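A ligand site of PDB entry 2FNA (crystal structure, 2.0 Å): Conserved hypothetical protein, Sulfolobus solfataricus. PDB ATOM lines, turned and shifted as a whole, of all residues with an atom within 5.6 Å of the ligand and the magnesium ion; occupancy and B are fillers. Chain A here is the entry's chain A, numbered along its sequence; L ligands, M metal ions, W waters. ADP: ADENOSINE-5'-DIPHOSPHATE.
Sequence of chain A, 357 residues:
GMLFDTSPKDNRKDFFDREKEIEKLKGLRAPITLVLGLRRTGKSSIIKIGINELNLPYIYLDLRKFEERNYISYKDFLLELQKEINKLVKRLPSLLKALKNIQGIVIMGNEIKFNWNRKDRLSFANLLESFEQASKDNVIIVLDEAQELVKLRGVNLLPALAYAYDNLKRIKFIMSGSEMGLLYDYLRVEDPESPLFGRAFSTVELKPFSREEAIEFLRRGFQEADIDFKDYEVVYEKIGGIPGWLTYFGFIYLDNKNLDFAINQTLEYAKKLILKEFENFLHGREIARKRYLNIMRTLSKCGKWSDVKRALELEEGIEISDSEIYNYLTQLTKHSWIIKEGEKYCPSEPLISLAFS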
ATOM      1  N   LEU A   3      -6.274  25.299   7.268  1.00  0.00           N
ATOM      2  CA  LEU A   3      -5.617  24.542   6.232  1.00  0.00           C
ATOM      3  C   LEU A   3      -5.742  23.012   6.401  1.00  0.00           C
ATOM      4  O   LEU A   3      -5.798  22.280   5.436  1.00  0.00           O
ATOM      5  CB  LEU A   3      -4.149  24.923   6.176  1.00  0.00           C
ATOM      6  CG  LEU A   3      -3.394  24.498   4.934  1.00  0.00           C
ATOM      7  CD1 LEU A   3      -3.864  25.384   3.754  1.00  0.00           C
ATOM      8  CD2 LEU A   3      -1.875  24.632   5.138  1.00  0.00           C
ATOM      9  N   ASP A   5      -8.313  21.289   7.931  1.00  0.00           N
ATOM     10  CA  ASP A   5      -9.646  20.678   8.037  1.00  0.00           C
ATOM     11  C   ASP A   5      -9.728  19.376   7.205  1.00  0.00           C
ATOM     12  O   ASP A   5      -9.368  19.332   6.015  1.00  0.00           O
ATOM     13  CB  ASP A   5     -10.751  21.646   7.581  1.00  0.00           C
ATOM     14  CG  ASP A   5     -10.947  22.816   8.520  1.00  0.00           C
ATOM     15  OD1 ASP A   5     -10.552  22.753   9.712  1.00  0.00           O
ATOM     16  OD2 ASP A   5     -11.532  23.815   8.061  1.00  0.00           O
ATOM     17  N   THR A   6     -10.157  18.305   7.853  1.00  0.00           N
ATOM     18  CA  THR A   6     -10.295  17.009   7.229  1.00  0.00           C
ATOM     19  C   THR A   6     -11.720  16.872   6.660  1.00  0.00           C
ATOM     20  O   THR A   6     -12.599  16.188   7.269  1.00  0.00           O
ATOM     21  CB  THR A   6     -10.050  15.861   8.259  1.00  0.00           C
ATOM     22  OG1 THR A   6     -11.028  15.951   9.296  1.00  0.00           O
ATOM     23  CG2 THR A   6      -8.617  15.929   8.837  1.00  0.00           C
ATOM     24  N   SER A   7     -11.935  17.591   5.585  1.00  0.00           N
ATOM     25  CA  SER A   7     -13.088  17.493   4.697  1.00  0.00           C
ATOM     26  C   SER A   7     -12.682  18.327   3.451  1.00  0.00           C
ATOM     27  O   SER A   7     -11.698  19.105   3.497  1.00  0.00           O
ATOM     28  CB  SER A   7     -14.410  17.963   5.337  1.00  0.00           C
ATOM     29  OG  SER A   7     -14.375  19.333   5.740  1.00  0.00           O
ATOM     30  N   PRO A   8     -13.348  18.101   2.302  1.00  0.00           N
ATOM     31  CA  PRO A   8     -13.007  18.945   1.177  1.00  0.00           C
ATOM     32  C   PRO A   8     -13.182  20.450   1.457  1.00  0.00           C
ATOM     33  O   PRO A   8     -14.170  20.863   2.051  1.00  0.00           O
ATOM     34  CB  PRO A   8     -13.976  18.432   0.088  1.00  0.00           C
ATOM     35  CG  PRO A   8     -14.143  16.978   0.447  1.00  0.00           C
ATOM     36  CD  PRO A   8     -14.355  17.097   1.927  1.00  0.00           C
ATOM     37  N   LYS A   9     -12.218  21.257   1.029  1.00  0.00           N
ATOM     38  CA  LYS A   9     -12.242  22.687   1.307  1.00  0.00           C
ATOM     39  C   LYS A   9     -13.253  23.301   0.372  1.00  0.00           C
ATOM     40  O   LYS A   9     -13.453  22.790  -0.735  1.00  0.00           O
ATOM     41  CB  LYS A   9     -10.868  23.333   1.079  1.00  0.00           C
ATOM     42  CG  LYS A   9      -9.720  22.734   1.931  1.00  0.00           C
ATOM     43  CD  LYS A   9     -10.021  22.737   3.433  1.00  0.00           C
ATOM     44  CE  LYS A   9      -8.714  22.624   4.256  1.00  0.00           C
ATOM     45  NZ  LYS A   9      -7.990  21.278   4.158  1.00  0.00           N
ATOM     46  N   ASP A  14      -8.608  28.592   2.745  1.00  0.00           N
ATOM     47  CA  ASP A  14      -8.280  27.364   3.466  1.00  0.00           C
ATOM     48  C   ASP A  14      -7.469  26.365   2.620  1.00  0.00           C
ATOM     49  O   ASP A  14      -7.270  25.239   3.027  1.00  0.00           O
ATOM     50  CB  ASP A  14      -9.562  26.673   3.915  1.00  0.00           C
ATOM     51  CG  ASP A  14     -10.442  27.540   4.814  1.00  0.00           C
ATOM     52  OD1 ASP A  14      -9.932  28.394   5.570  1.00  0.00           O
ATOM     53  OD2 ASP A  14     -11.682  27.348   4.796  1.00  0.00           O
ATOM     54  N   PHE A  15      -6.980  26.779   1.446  1.00  0.00           N
ATOM     55  CA  PHE A  15      -6.489  25.856   0.479  1.00  0.00           C
ATOM     56  C   PHE A  15      -5.127  26.281  -0.023  1.00  0.00           C
ATOM     57  O   PHE A  15      -4.957  27.391  -0.467  1.00  0.00           O
ATOM     58  CB  PHE A  15      -7.521  25.784  -0.653  1.00  0.00           C
ATOM     59  CG  PHE A  15      -7.375  24.630  -1.570  1.00  0.00           C
ATOM     60  CD1 PHE A  15      -7.838  23.359  -1.192  1.00  0.00           C
ATOM     61  CD2 PHE A  15      -6.799  24.790  -2.836  1.00  0.00           C
ATOM     62  CE1 PHE A  15      -7.717  22.298  -2.049  1.00  0.00           C
ATOM     63  CE2 PHE A  15      -6.683  23.727  -3.684  1.00  0.00           C
ATOM     64  CZ  PHE A  15      -7.150  22.457  -3.285  1.00  0.00           C
ATOM     65  N   PHE A  16      -4.144  25.382   0.055  1.00  0.00           N
ATOM     66  CA  PHE A  16      -2.764  25.663  -0.406  1.00  0.00           C
ATOM     67  C   PHE A  16      -2.598  25.640  -1.934  1.00  0.00           C
ATOM     68  O   PHE A  16      -2.792  24.595  -2.555  1.00  0.00           O
ATOM     69  CB  PHE A  16      -1.820  24.630   0.175  1.00  0.00           C
ATOM     70  CG  PHE A  16      -0.408  24.773  -0.270  1.00  0.00           C
ATOM     71  CD1 PHE A  16       0.319  25.921   0.052  1.00  0.00           C
ATOM     72  CD2 PHE A  16       0.240  23.754  -0.944  1.00  0.00           C
ATOM     73  CE1 PHE A  16       1.627  26.032  -0.333  1.00  0.00           C
ATOM     74  CE2 PHE A  16       1.560  23.863  -1.322  1.00  0.00           C
ATOM     75  CZ  PHE A  16       2.256  24.996  -1.023  1.00  0.00           C
ATOM     76  N   ASP A  17      -2.198  26.778  -2.508  1.00  0.00           N
ATOM     77  CA  ASP A  17      -1.940  26.970  -3.943  1.00  0.00           C
ATOM     78  C   ASP A  17      -2.938  26.298  -4.867  1.00  0.00           C
ATOM     79  O   ASP A  17      -4.131  26.573  -4.746  1.00  0.00           O
ATOM     80  CB  ASP A  17      -0.479  26.627  -4.319  1.00  0.00           C
ATOM     81  CG  ASP A  17       0.038  27.434  -5.554  1.00  0.00           C
ATOM     82  OD1 ASP A  17      -0.749  28.098  -6.316  1.00  0.00           O
ATOM     83  OD2 ASP A  17       1.278  27.411  -5.754  1.00  0.00           O
ATOM     84  N   ARG A  18      -2.448  25.447  -5.779  1.00  0.00           N
ATOM     85  CA  ARG A  18      -3.180  25.045  -6.982  1.00  0.00           C
ATOM     86  C   ARG A  18      -3.885  26.199  -7.708  1.00  0.00           C
ATOM     87  O   ARG A  18      -4.966  26.010  -8.267  1.00  0.00           O
ATOM     88  CB  ARG A  18      -4.227  23.951  -6.675  1.00  0.00           C
ATOM     89  CG  ARG A  18      -3.744  22.853  -5.824  1.00  0.00           C
ATOM     90  CD  ARG A  18      -2.677  21.958  -6.463  1.00  0.00           C
ATOM     91  NE  ARG A  18      -2.774  20.654  -5.840  1.00  0.00           N
ATOM     92  CZ  ARG A  18      -1.877  19.684  -5.941  1.00  0.00           C
ATOM     93  NH1 ARG A  18      -0.775  19.859  -6.659  1.00  0.00           N
ATOM     94  NH2 ARG A  18      -2.124  18.516  -5.344  1.00  0.00           N
ATOM     95  N   GLY A  37      -6.870  13.342 -11.154  1.00  0.00           N
ATOM     96  CA  GLY A  37      -6.007  13.225  -9.998  1.00  0.00           C
ATOM     97  C   GLY A  37      -6.373  12.002  -9.188  1.00  0.00           C
ATOM     98  O   GLY A  37      -7.519  11.597  -9.163  1.00  0.00           O
ATOM     99  N   LEU A  38      -5.371  11.394  -8.546  1.00  0.00           N
ATOM    100  CA  LEU A  38      -5.631  10.281  -7.641  1.00  0.00           C
ATOM    101  C   LEU A  38      -6.542  10.716  -6.525  1.00  0.00           C
ATOM    102  O   LEU A  38      -6.671  11.928  -6.230  1.00  0.00           O
ATOM    103  CB  LEU A  38      -4.326   9.773  -7.029  1.00  0.00           C
ATOM    104  CG  LEU A  38      -3.320   9.177  -8.026  1.00  0.00           C
ATOM    105  CD1 LEU A  38      -1.874   9.112  -7.395  1.00  0.00           C
ATOM    106  CD2 LEU A  38      -3.734   7.835  -8.504  1.00  0.00           C
ATOM    107  N   ARG A  39      -7.164   9.751  -5.879  1.00  0.00           N
ATOM    108  CA  ARG A  39      -7.863  10.047  -4.675  1.00  0.00           C
ATOM    109  C   ARG A  39      -7.041  10.927  -3.750  1.00  0.00           C
ATOM    110  O   ARG A  39      -5.828  10.786  -3.627  1.00  0.00           O
ATOM    111  CB  ARG A  39      -8.257   8.791  -3.928  1.00  0.00           C
ATOM    112  CG  ARG A  39      -9.510   8.194  -4.394  1.00  0.00           C
ATOM    113  CD  ARG A  39      -9.904   7.038  -3.510  1.00  0.00           C
ATOM    114  NE  ARG A  39     -10.337   5.939  -4.338  1.00  0.00           N
ATOM    115  CZ  ARG A  39     -11.482   5.899  -5.000  1.00  0.00           C
ATOM    116  NH1 ARG A  39     -12.363   6.893  -4.906  1.00  0.00           N
ATOM    117  NH2 ARG A  39     -11.745   4.841  -5.750  1.00  0.00           N
ATOM    118  N   ARG A  40      -7.743  11.861  -3.109  1.00  0.00           N
ATOM    119  CA  ARG A  40      -7.188  12.723  -2.060  1.00  0.00           C
ATOM    120  C   ARG A  40      -6.192  13.750  -2.536  1.00  0.00           C
ATOM    121  O   ARG A  40      -5.389  14.250  -1.743  1.00  0.00           O
ATOM    122  CB  ARG A  40      -6.608  11.874  -0.936  1.00  0.00           C
ATOM    123  CG  ARG A  40      -7.672  11.236  -0.124  1.00  0.00           C
ATOM    124  CD  ARG A  40      -7.066  10.221   0.812  1.00  0.00           C
ATOM    125  NE  ARG A  40      -6.659   8.978   0.134  1.00  0.00           N
ATOM    126  CZ  ARG A  40      -7.485   8.013  -0.231  1.00  0.00           C
ATOM    127  NH1 ARG A  40      -8.800   8.111  -0.005  1.00  0.00           N
ATOM    128  NH2 ARG A  40      -7.012   6.918  -0.790  1.00  0.00           N
ATOM    129  N   THR A  41      -6.309  14.127  -3.807  1.00  0.00           N
ATOM    130  CA  THR A  41      -5.433  15.158  -4.390  1.00  0.00           C
ATOM    131  C   THR A  41      -6.088  16.557  -4.429  1.00  0.00           C
ATOM    132  O   THR A  41      -5.440  17.527  -4.794  1.00  0.00           O
ATOM    133  CB  THR A  41      -4.879  14.755  -5.796  1.00  0.00           C
ATOM    134  OG1 THR A  41      -5.943  14.340  -6.637  1.00  0.00           O
ATOM    135  CG2 THR A  41      -3.848  13.607  -5.676  1.00  0.00           C
ATOM    136  N   GLY A  42      -7.353  16.659  -4.041  1.00  0.00           N
ATOM    137  CA  GLY A  42      -8.037  17.936  -3.916  1.00  0.00           C
ATOM    138  C   GLY A  42      -9.051  18.220  -4.982  1.00  0.00           C
ATOM    139  O   GLY A  42      -9.465  19.388  -5.147  1.00  0.00           O
ATOM    140  N   LYS A  43      -9.481  17.190  -5.717  1.00  0.00           N
ATOM    141  CA  LYS A  43     -10.380  17.408  -6.865  1.00  0.00           C
ATOM    142  C   LYS A  43     -11.705  17.989  -6.376  1.00  0.00           C
ATOM    143  O   LYS A  43     -12.124  19.022  -6.858  1.00  0.00           O
ATOM    144  CB  LYS A  43     -10.628  16.123  -7.671  1.00  0.00           C
ATOM    145  CG  LYS A  43      -9.392  15.496  -8.324  1.00  0.00           C
ATOM    146  CD  LYS A  43      -9.743  14.251  -9.109  1.00  0.00           C
ATOM    147  CE  LYS A  43     -10.313  13.110  -8.242  1.00  0.00           C
ATOM    148  NZ  LYS A  43      -9.349  12.637  -7.235  1.00  0.00           N
ATOM    149  N   SER A  44     -12.360  17.349  -5.403  1.00  0.00           N
ATOM    150  CA  SER A  44     -13.651  17.866  -4.923  1.00  0.00           C
ATOM    151  C   SER A  44     -13.471  19.276  -4.338  1.00  0.00           C
ATOM    152  O   SER A  44     -14.342  20.140  -4.528  1.00  0.00           O
ATOM    153  CB  SER A  44     -14.321  16.914  -3.918  1.00  0.00           C
ATOM    154  OG  SER A  44     -14.610  15.626  -4.486  1.00  0.00           O
ATOM    155  N   SER A  45     -12.355  19.515  -3.649  1.00  0.00           N
ATOM    156  CA  SER A  45     -12.012  20.850  -3.119  1.00  0.00           C
ATOM    157  C   SER A  45     -11.958  21.968  -4.182  1.00  0.00           C
ATOM    158  O   SER A  45     -12.589  23.053  -4.008  1.00  0.00           O
ATOM    159  CB  SER A  45     -10.685  20.798  -2.326  1.00  0.00           C
ATOM    160  OG  SER A  45     -10.731  19.900  -1.207  1.00  0.00           O
ATOM    161  N   ILE A  46     -11.214  21.767  -5.259  1.00  0.00           N
ATOM    162  CA  ILE A  46     -11.106  22.852  -6.239  1.00  0.00           C
ATOM    163  C   ILE A  46     -12.413  23.081  -6.981  1.00  0.00           C
ATOM    164  O   ILE A  46     -12.683  24.189  -7.400  1.00  0.00           O
ATOM    165  CB  ILE A  46      -9.964  22.685  -7.272  1.00  0.00           C
ATOM    166  CG1 ILE A  46     -10.135  21.456  -8.172  1.00  0.00           C
ATOM    167  CG2 ILE A  46      -8.626  22.724  -6.591  1.00  0.00           C
ATOM    168  CD1 ILE A  46      -9.335  21.592  -9.467  1.00  0.00           C
ATOM    169  N   ARG A  64     -19.639   9.536  -5.361  1.00  0.00           N
ATOM    170  CA  ARG A  64     -18.900   8.745  -4.389  1.00  0.00           C
ATOM    171  C   ARG A  64     -19.845   7.953  -3.514  1.00  0.00           C
ATOM    172  O   ARG A  64     -19.465   6.907  -3.011  1.00  0.00           O
ATOM    173  CB  ARG A  64     -18.072   9.644  -3.454  1.00  0.00           C
ATOM    174  CG  ARG A  64     -16.565   9.609  -3.653  1.00  0.00           C
ATOM    175  CD  ARG A  64     -15.777   9.440  -2.317  1.00  0.00           C
ATOM    176  NE  ARG A  64     -16.381  10.131  -1.159  1.00  0.00           N
ATOM    177  N   ASP A 144     -19.210  14.550  -9.846  1.00  0.00           N
ATOM    178  CA  ASP A 144     -18.026  14.337  -9.054  1.00  0.00           C
ATOM    179  C   ASP A 144     -17.853  12.824  -8.857  1.00  0.00           C
ATOM    180  O   ASP A 144     -18.645  12.178  -8.184  1.00  0.00           O
ATOM    181  CB  ASP A 144     -18.123  15.100  -7.740  1.00  0.00           C
ATOM    182  CG  ASP A 144     -16.795  15.210  -6.972  1.00  0.00           C
ATOM    183  OD1 ASP A 144     -15.748  14.723  -7.445  1.00  0.00           O
ATOM    184  OD2 ASP A 144     -16.833  15.794  -5.854  1.00  0.00           O
ATOM    185  N   GLU A 145     -16.795  12.321  -9.472  1.00  0.00           N
ATOM    186  CA  GLU A 145     -16.526  10.877  -9.666  1.00  0.00           C
ATOM    187  C   GLU A 145     -17.446  10.277 -10.738  1.00  0.00           C
ATOM    188  O   GLU A 145     -18.108   9.272 -10.524  1.00  0.00           O
ATOM    189  CB  GLU A 145     -16.555  10.090  -8.348  1.00  0.00           C
ATOM    190  CG  GLU A 145     -15.485  10.544  -7.312  1.00  0.00           C
ATOM    191  CD  GLU A 145     -14.057  10.260  -7.715  1.00  0.00           C
ATOM    192  OE1 GLU A 145     -13.791   9.353  -8.549  1.00  0.00           O
ATOM    193  OE2 GLU A 145     -13.157  10.963  -7.213  1.00  0.00           O
ATOM    194  N   SER A 178     -11.176   9.948  -9.956  1.00  0.00           N
ATOM    195  CA  SER A 178      -9.982   9.454  -9.286  1.00  0.00           C
ATOM    196  C   SER A 178      -9.361   8.277 -10.021  1.00  0.00           C
ATOM    197  O   SER A 178      -8.253   7.910  -9.703  1.00  0.00           O
ATOM    198  CB  SER A 178     -10.306   9.033  -7.849  1.00  0.00           C
ATOM    199  OG  SER A 178     -10.633  10.178  -7.066  1.00  0.00           O
ATOM    200  N   LEU A 206      -4.678  17.170 -10.757  1.00  0.00           N
ATOM    201  CA  LEU A 206      -4.007  17.421  -9.490  1.00  0.00           C
ATOM    202  C   LEU A 206      -3.037  16.290  -9.150  1.00  0.00           C
ATOM    203  O   LEU A 206      -3.439  15.135  -8.966  1.00  0.00           O
ATOM    204  CB  LEU A 206      -5.032  17.574  -8.391  1.00  0.00           C
ATOM    205  CG  LEU A 206      -5.987  18.759  -8.563  1.00  0.00           C
ATOM    206  CD1 LEU A 206      -7.032  18.708  -7.522  1.00  0.00           C
ATOM    207  CD2 LEU A 206      -5.225  20.034  -8.472  1.00  0.00           C
ATOM    208  N   PHE A 209       1.658  16.353  -4.035  1.00  0.00           N
ATOM    209  CA  PHE A 209       2.737  17.292  -3.767  1.00  0.00           C
ATOM    210  C   PHE A 209       4.111  16.681  -3.983  1.00  0.00           C
ATOM    211  O   PHE A 209       4.379  15.529  -3.590  1.00  0.00           O
ATOM    212  CB  PHE A 209       2.640  17.832  -2.348  1.00  0.00           C
ATOM    213  CG  PHE A 209       1.374  18.641  -2.058  1.00  0.00           C
ATOM    214  CD1 PHE A 209       0.835  19.491  -2.990  1.00  0.00           C
ATOM    215  CD2 PHE A 209       0.784  18.581  -0.808  1.00  0.00           C
ATOM    216  CE1 PHE A 209      -0.314  20.238  -2.695  1.00  0.00           C
ATOM    217  CE2 PHE A 209      -0.353  19.340  -0.503  1.00  0.00           C
ATOM    218  CZ  PHE A 209      -0.887  20.179  -1.446  1.00  0.00           C
ATOM    219  N   PHE A 217       3.365  23.160   2.272  1.00  0.00           N
ATOM    220  CA  PHE A 217       1.965  23.002   2.720  1.00  0.00           C
ATOM    221  C   PHE A 217       1.892  22.916   4.237  1.00  0.00           C
ATOM    222  O   PHE A 217       1.080  23.588   4.892  1.00  0.00           O
ATOM    223  CB  PHE A 217       1.389  21.720   2.067  1.00  0.00           C
ATOM    224  CG  PHE A 217       0.053  21.308   2.600  1.00  0.00           C
ATOM    225  CD1 PHE A 217      -1.067  22.070   2.340  1.00  0.00           C
ATOM    226  CD2 PHE A 217      -0.093  20.143   3.354  1.00  0.00           C
ATOM    227  CE1 PHE A 217      -2.306  21.721   2.806  1.00  0.00           C
ATOM    228  CE2 PHE A 217      -1.331  19.769   3.826  1.00  0.00           C
ATOM    229  CZ  PHE A 217      -2.457  20.564   3.559  1.00  0.00           C
ATOM    230  N   PRO A 243      -2.049  15.016  -0.818  1.00  0.00           N
ATOM    231  CA  PRO A 243      -2.504  16.104   0.063  1.00  0.00           C
ATOM    232  C   PRO A 243      -3.406  15.687   1.215  1.00  0.00           C
ATOM    233  O   PRO A 243      -3.265  16.228   2.321  1.00  0.00           O
ATOM    234  CB  PRO A 243      -3.245  17.061  -0.898  1.00  0.00           C
ATOM    235  CG  PRO A 243      -2.557  16.869  -2.199  1.00  0.00           C
ATOM    236  CD  PRO A 243      -2.255  15.350  -2.238  1.00  0.00           C
ATOM    237  N   GLY A 244      -4.335  14.785   0.940  1.00  0.00           N
ATOM    238  CA  GLY A 244      -5.273  14.302   1.943  1.00  0.00           C
ATOM    239  C   GLY A 244      -4.602  13.688   3.142  1.00  0.00           C
ATOM    240  O   GLY A 244      -5.067  13.872   4.285  1.00  0.00           O
ATOM    241  N   TRP A 245      -3.509  12.952   2.937  1.00  0.00           N
ATOM    242  CA  TRP A 245      -2.832  12.320   4.074  1.00  0.00           C
ATOM    243  C   TRP A 245      -2.025  13.371   4.872  1.00  0.00           C
ATOM    244  O   TRP A 245      -1.950  13.313   6.113  1.00  0.00           O
ATOM    245  CB  TRP A 245      -1.884  11.228   3.632  1.00  0.00           C
ATOM    246  CG  TRP A 245      -2.438  10.084   2.863  1.00  0.00           C
ATOM    247  CD1 TRP A 245      -1.841   9.497   1.827  1.00  0.00           C
ATOM    248  CD2 TRP A 245      -3.670   9.355   3.091  1.00  0.00           C
ATOM    249  NE1 TRP A 245      -2.582   8.455   1.371  1.00  0.00           N
ATOM    250  CE2 TRP A 245      -3.711   8.342   2.127  1.00  0.00           C
ATOM    251  CE3 TRP A 245      -4.712   9.451   4.008  1.00  0.00           C
ATOM    252  CZ2 TRP A 245      -4.761   7.431   2.040  1.00  0.00           C
ATOM    253  CZ3 TRP A 245      -5.768   8.534   3.915  1.00  0.00           C
ATOM    254  CH2 TRP A 245      -5.780   7.544   2.950  1.00  0.00           C
ATOM    255  N   THR A 247      -2.777  16.515   5.121  1.00  0.00           N
ATOM    256  CA  THR A 247      -3.825  17.268   5.814  1.00  0.00           C
ATOM    257  C   THR A 247      -4.244  16.616   7.141  1.00  0.00           C
ATOM    258  O   THR A 247      -4.346  17.295   8.140  1.00  0.00           O
ATOM    259  CB  THR A 247      -5.077  17.397   4.909  1.00  0.00           C
ATOM    260  OG1 THR A 247      -4.729  18.040   3.693  1.00  0.00           O
ATOM    261  CG2 THR A 247      -6.228  18.229   5.563  1.00  0.00           C
HETATM  262  PB  ADP L   1     -10.283  14.274  -3.926  1.00  0.00           P
HETATM  263  O1B ADP L   1      -9.266  14.502  -4.992  1.00  0.00           O
HETATM  264  O2B ADP L   1     -10.210  12.864  -3.350  1.00  0.00           O
HETATM  265  O3B ADP L   1     -11.666  14.756  -4.196  1.00  0.00           O
HETATM  266  PA  ADP L   1     -10.476  16.159  -1.662  1.00  0.00           P
HETATM  267  O1A ADP L   1     -10.894  17.486  -2.216  1.00  0.00           O
HETATM  268  O2A ADP L   1     -11.607  15.429  -1.085  1.00  0.00           O
HETATM  269  O3A ADP L   1      -9.664  15.195  -2.677  1.00  0.00           O
HETATM  270  O5' ADP L   1      -9.275  16.453  -0.665  1.00  0.00           O
HETATM  271  C5' ADP L   1      -8.732  15.456   0.214  1.00  0.00           C
HETATM  272  C4' ADP L   1      -8.333  16.082   1.546  1.00  0.00           C
HETATM  273  O4' ADP L   1      -7.155  16.853   1.429  1.00  0.00           O
HETATM  274  C3' ADP L   1      -9.361  17.020   2.112  1.00  0.00           C
HETATM  275  O3' ADP L   1      -9.198  16.999   3.548  1.00  0.00           O
HETATM  276  C2' ADP L   1      -8.933  18.384   1.620  1.00  0.00           C
HETATM  277  O2' ADP L   1      -9.350  19.434   2.477  1.00  0.00           O
HETATM  278  C1' ADP L   1      -7.442  18.226   1.664  1.00  0.00           C
HETATM  279  N9  ADP L   1      -6.695  18.953   0.640  1.00  0.00           N
HETATM  280  C8  ADP L   1      -6.337  18.473  -0.569  1.00  0.00           C
HETATM  281  N7  ADP L   1      -5.605  19.380  -1.226  1.00  0.00           N
HETATM  282  C5  ADP L   1      -5.506  20.471  -0.432  1.00  0.00           C
HETATM  283  C6  ADP L   1      -4.864  21.804  -0.505  1.00  0.00           C
HETATM  284  N6  ADP L   1      -4.178  22.180  -1.607  1.00  0.00           N
HETATM  285  N1  ADP L   1      -4.967  22.637   0.573  1.00  0.00           N
HETATM  286  C2  ADP L   1      -5.637  22.289   1.681  1.00  0.00           C
HETATM  287  N3  ADP L   1      -6.233  21.091   1.820  1.00  0.00           N
HETATM  288  C4  ADP L   1      -6.192  20.172   0.811  1.00  0.00           C
HETATM  289 MG    MG M   1     -13.459  13.831  -4.228  1.00  0.00          MG
HETATM  290  O   HOH W   1      -4.568  19.749  -3.620  1.00  0.00           O
HETATM  291  O   HOH W   2     -12.530  11.937  -3.999  1.00  0.00           O
HETATM  292  O   HOH W   3     -13.591  14.202  -2.159  1.00  0.00           O
HETATM  293  O   HOH W   4     -15.386  12.941  -4.126  1.00  0.00           O
HETATM  294  O   HOH W   5     -13.641  13.667  -6.209  1.00  0.00           O
HETATM  295  O   HOH W   6     -11.055  12.087  -0.706  1.00  0.00           O
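An oxygen (O3B) of the ligand sits close to the backbone NH of Ser 44, 2.9 Å away.
N of Ser 7 is in hydrogen-bond range of O3' of the ligand.
An oxygen (O2') of the ligand lies within hydrogen-bond range of the backbone carbonyl oxygen (O) of Ser 7 (2.6 Å).
O1A of the ligand lies within hydrogen-bond range of N of Ser 45, at 2.9 Å.
O1A of the ligand sits at hydrogen-bond distance from OG of Ser 45.
An oxygen (O2B) of the ligand sits at hydrogen-bond distance from the backbone NH of Arg 40.
N of Lys 43 sits at hydrogen-bond distance from O1B of the ligand, at 2.8 Å.
The side-chain amino group (NZ) of Lys 43 lies within salt-bridge range of an oxygen (O1B) of the ligand (2.9 Å).
The side-chain amino group of Lys 9 lies within hydrogen-bond range of an oxygen (O2') of the ligand, at 2.8 Å.
N of Phe 16 lies within hydrogen-bond range of N1 of the ligand.
O of Phe 16 sits at hydrogen-bond distance from N6 of the ligand, 2.9 Å away.
The backbone NH of Gly 42 sits at hydrogen-bond distance from an oxygen (O1B) of the ligand.
An oxygen (O1B) of the ligand lies within hydrogen-bond range of the backbone NH of Thr 41, 3.2 Å away.
The backbone carbonyl oxygen (O) of Asp 5 is in hydrogen-bond range of an oxygen (O3') of the ligand (3.4 Å).
The side-chain hydroxyl (OG) of Ser 44 sits close to the side-chain carboxylate (OD2) of Asp 144, at 2.6 Å.
The side-chain hydroxyl of Ser 45 lies within hydrogen-bond range of the backbone NH of Lys 9.
The backbone NH of Gly 244 sits at hydrogen-bond distance from the backbone carbonyl oxygen of Arg 40, at 2.9 Å.
The side-chain amino group (NZ) of Lys 43 lies within hydrogen-bond range of the side-chain hydroxyl (OG) of Ser 178 (2.8 Å).
The side-chain amino group (NZ) of Lys 43 is in hydrogen-bond range of the backbone carbonyl oxygen (O) of Gly 37.
The side-chain amino group of Lys 9 lies within hydrogen-bond range of the backbone carbonyl oxygen of Leu 3 (2.7 Å).
O of Leu 38 is in hydrogen-bond range of OG1 of Thr 41 (2.6 Å).
The backbone carbonyl oxygen (O) of Pro 243 is in hydrogen-bond range of the side-chain hydroxyl (OG1) of Thr 247 (2.7 Å).
Leu 3 touches the ligand.
Thr 6 touches the ligand (CA to O3', 3.8 Å).
CG of Pro 8 touches O2A of the ligand, at 3.3 Å.
Asp 14 touches the ligand.
Phe 15 touches the ligand.
O of Leu 38 touches O1B of the ligand (3.9 Å).
C of Arg 39 touches O2B of the ligand, at 3.7 Å.
CZ of Phe 209 touches N6 of the ligand, 3.9 Å away.
CE1 of Phe 217 touches C2 of the ligand, 3.6 Å away.
Pro 243 touches the ligand.
Gly 244 touches the ligand.
Thr 247 touches the ligand.
Hydrophobic or aromatic side chains within 4 Å of the ligand: Pro 8, Phe 15, Phe 16, Phe 209, Phe 217 and Pro 243.
Within 4 Å of the ligand: Leu 3, Asp 5, Thr 6, Ser 7, Pro 8, Lys 9, Asp 14, Phe 15, Phe 16, Leu 38, Arg 39, Arg 40, Thr 41, Gly 42, Lys 43, Ser 44, Ser 45, Phe 209, Phe 217, Pro 243, Gly 244 and Thr 247.
The nearest printed residue that does not touch the ligand is Arg 18 (4.3 Å).
Of the 32 residues printed, 1 comes within 4 Å of the magnesium ion.
The magnesium ion is bound by water W5, at 2.0 Å.
The magnesium ion is bound by O3B of the ligand, at 2.0 Å.
The magnesium ion is bound by water W3 (2.1 Å).
The magnesium ion is bound by water W2 (2.1 Å).
The magnesium ion is bound by water W4.
The magnesium ion is bound by OG of Ser 44.
The magnesium ion has six donor atoms within binding distance.
Water W2 lies within hydrogen-bond range of O2B of the ligand (2.6 Å) and OE2 of Glu 145 (3.4 Å).
Water W5 lies within hydrogen-bond range of the side-chain carboxylate of Asp 144 and the side-chain carboxylate of Glu 145.
Water W1 lies within hydrogen-bond range of a nitrogen (N7) of the ligand, the backbone carbonyl oxygen (O) of Thr 41 and the guanidinium group (NE) of Arg 18.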
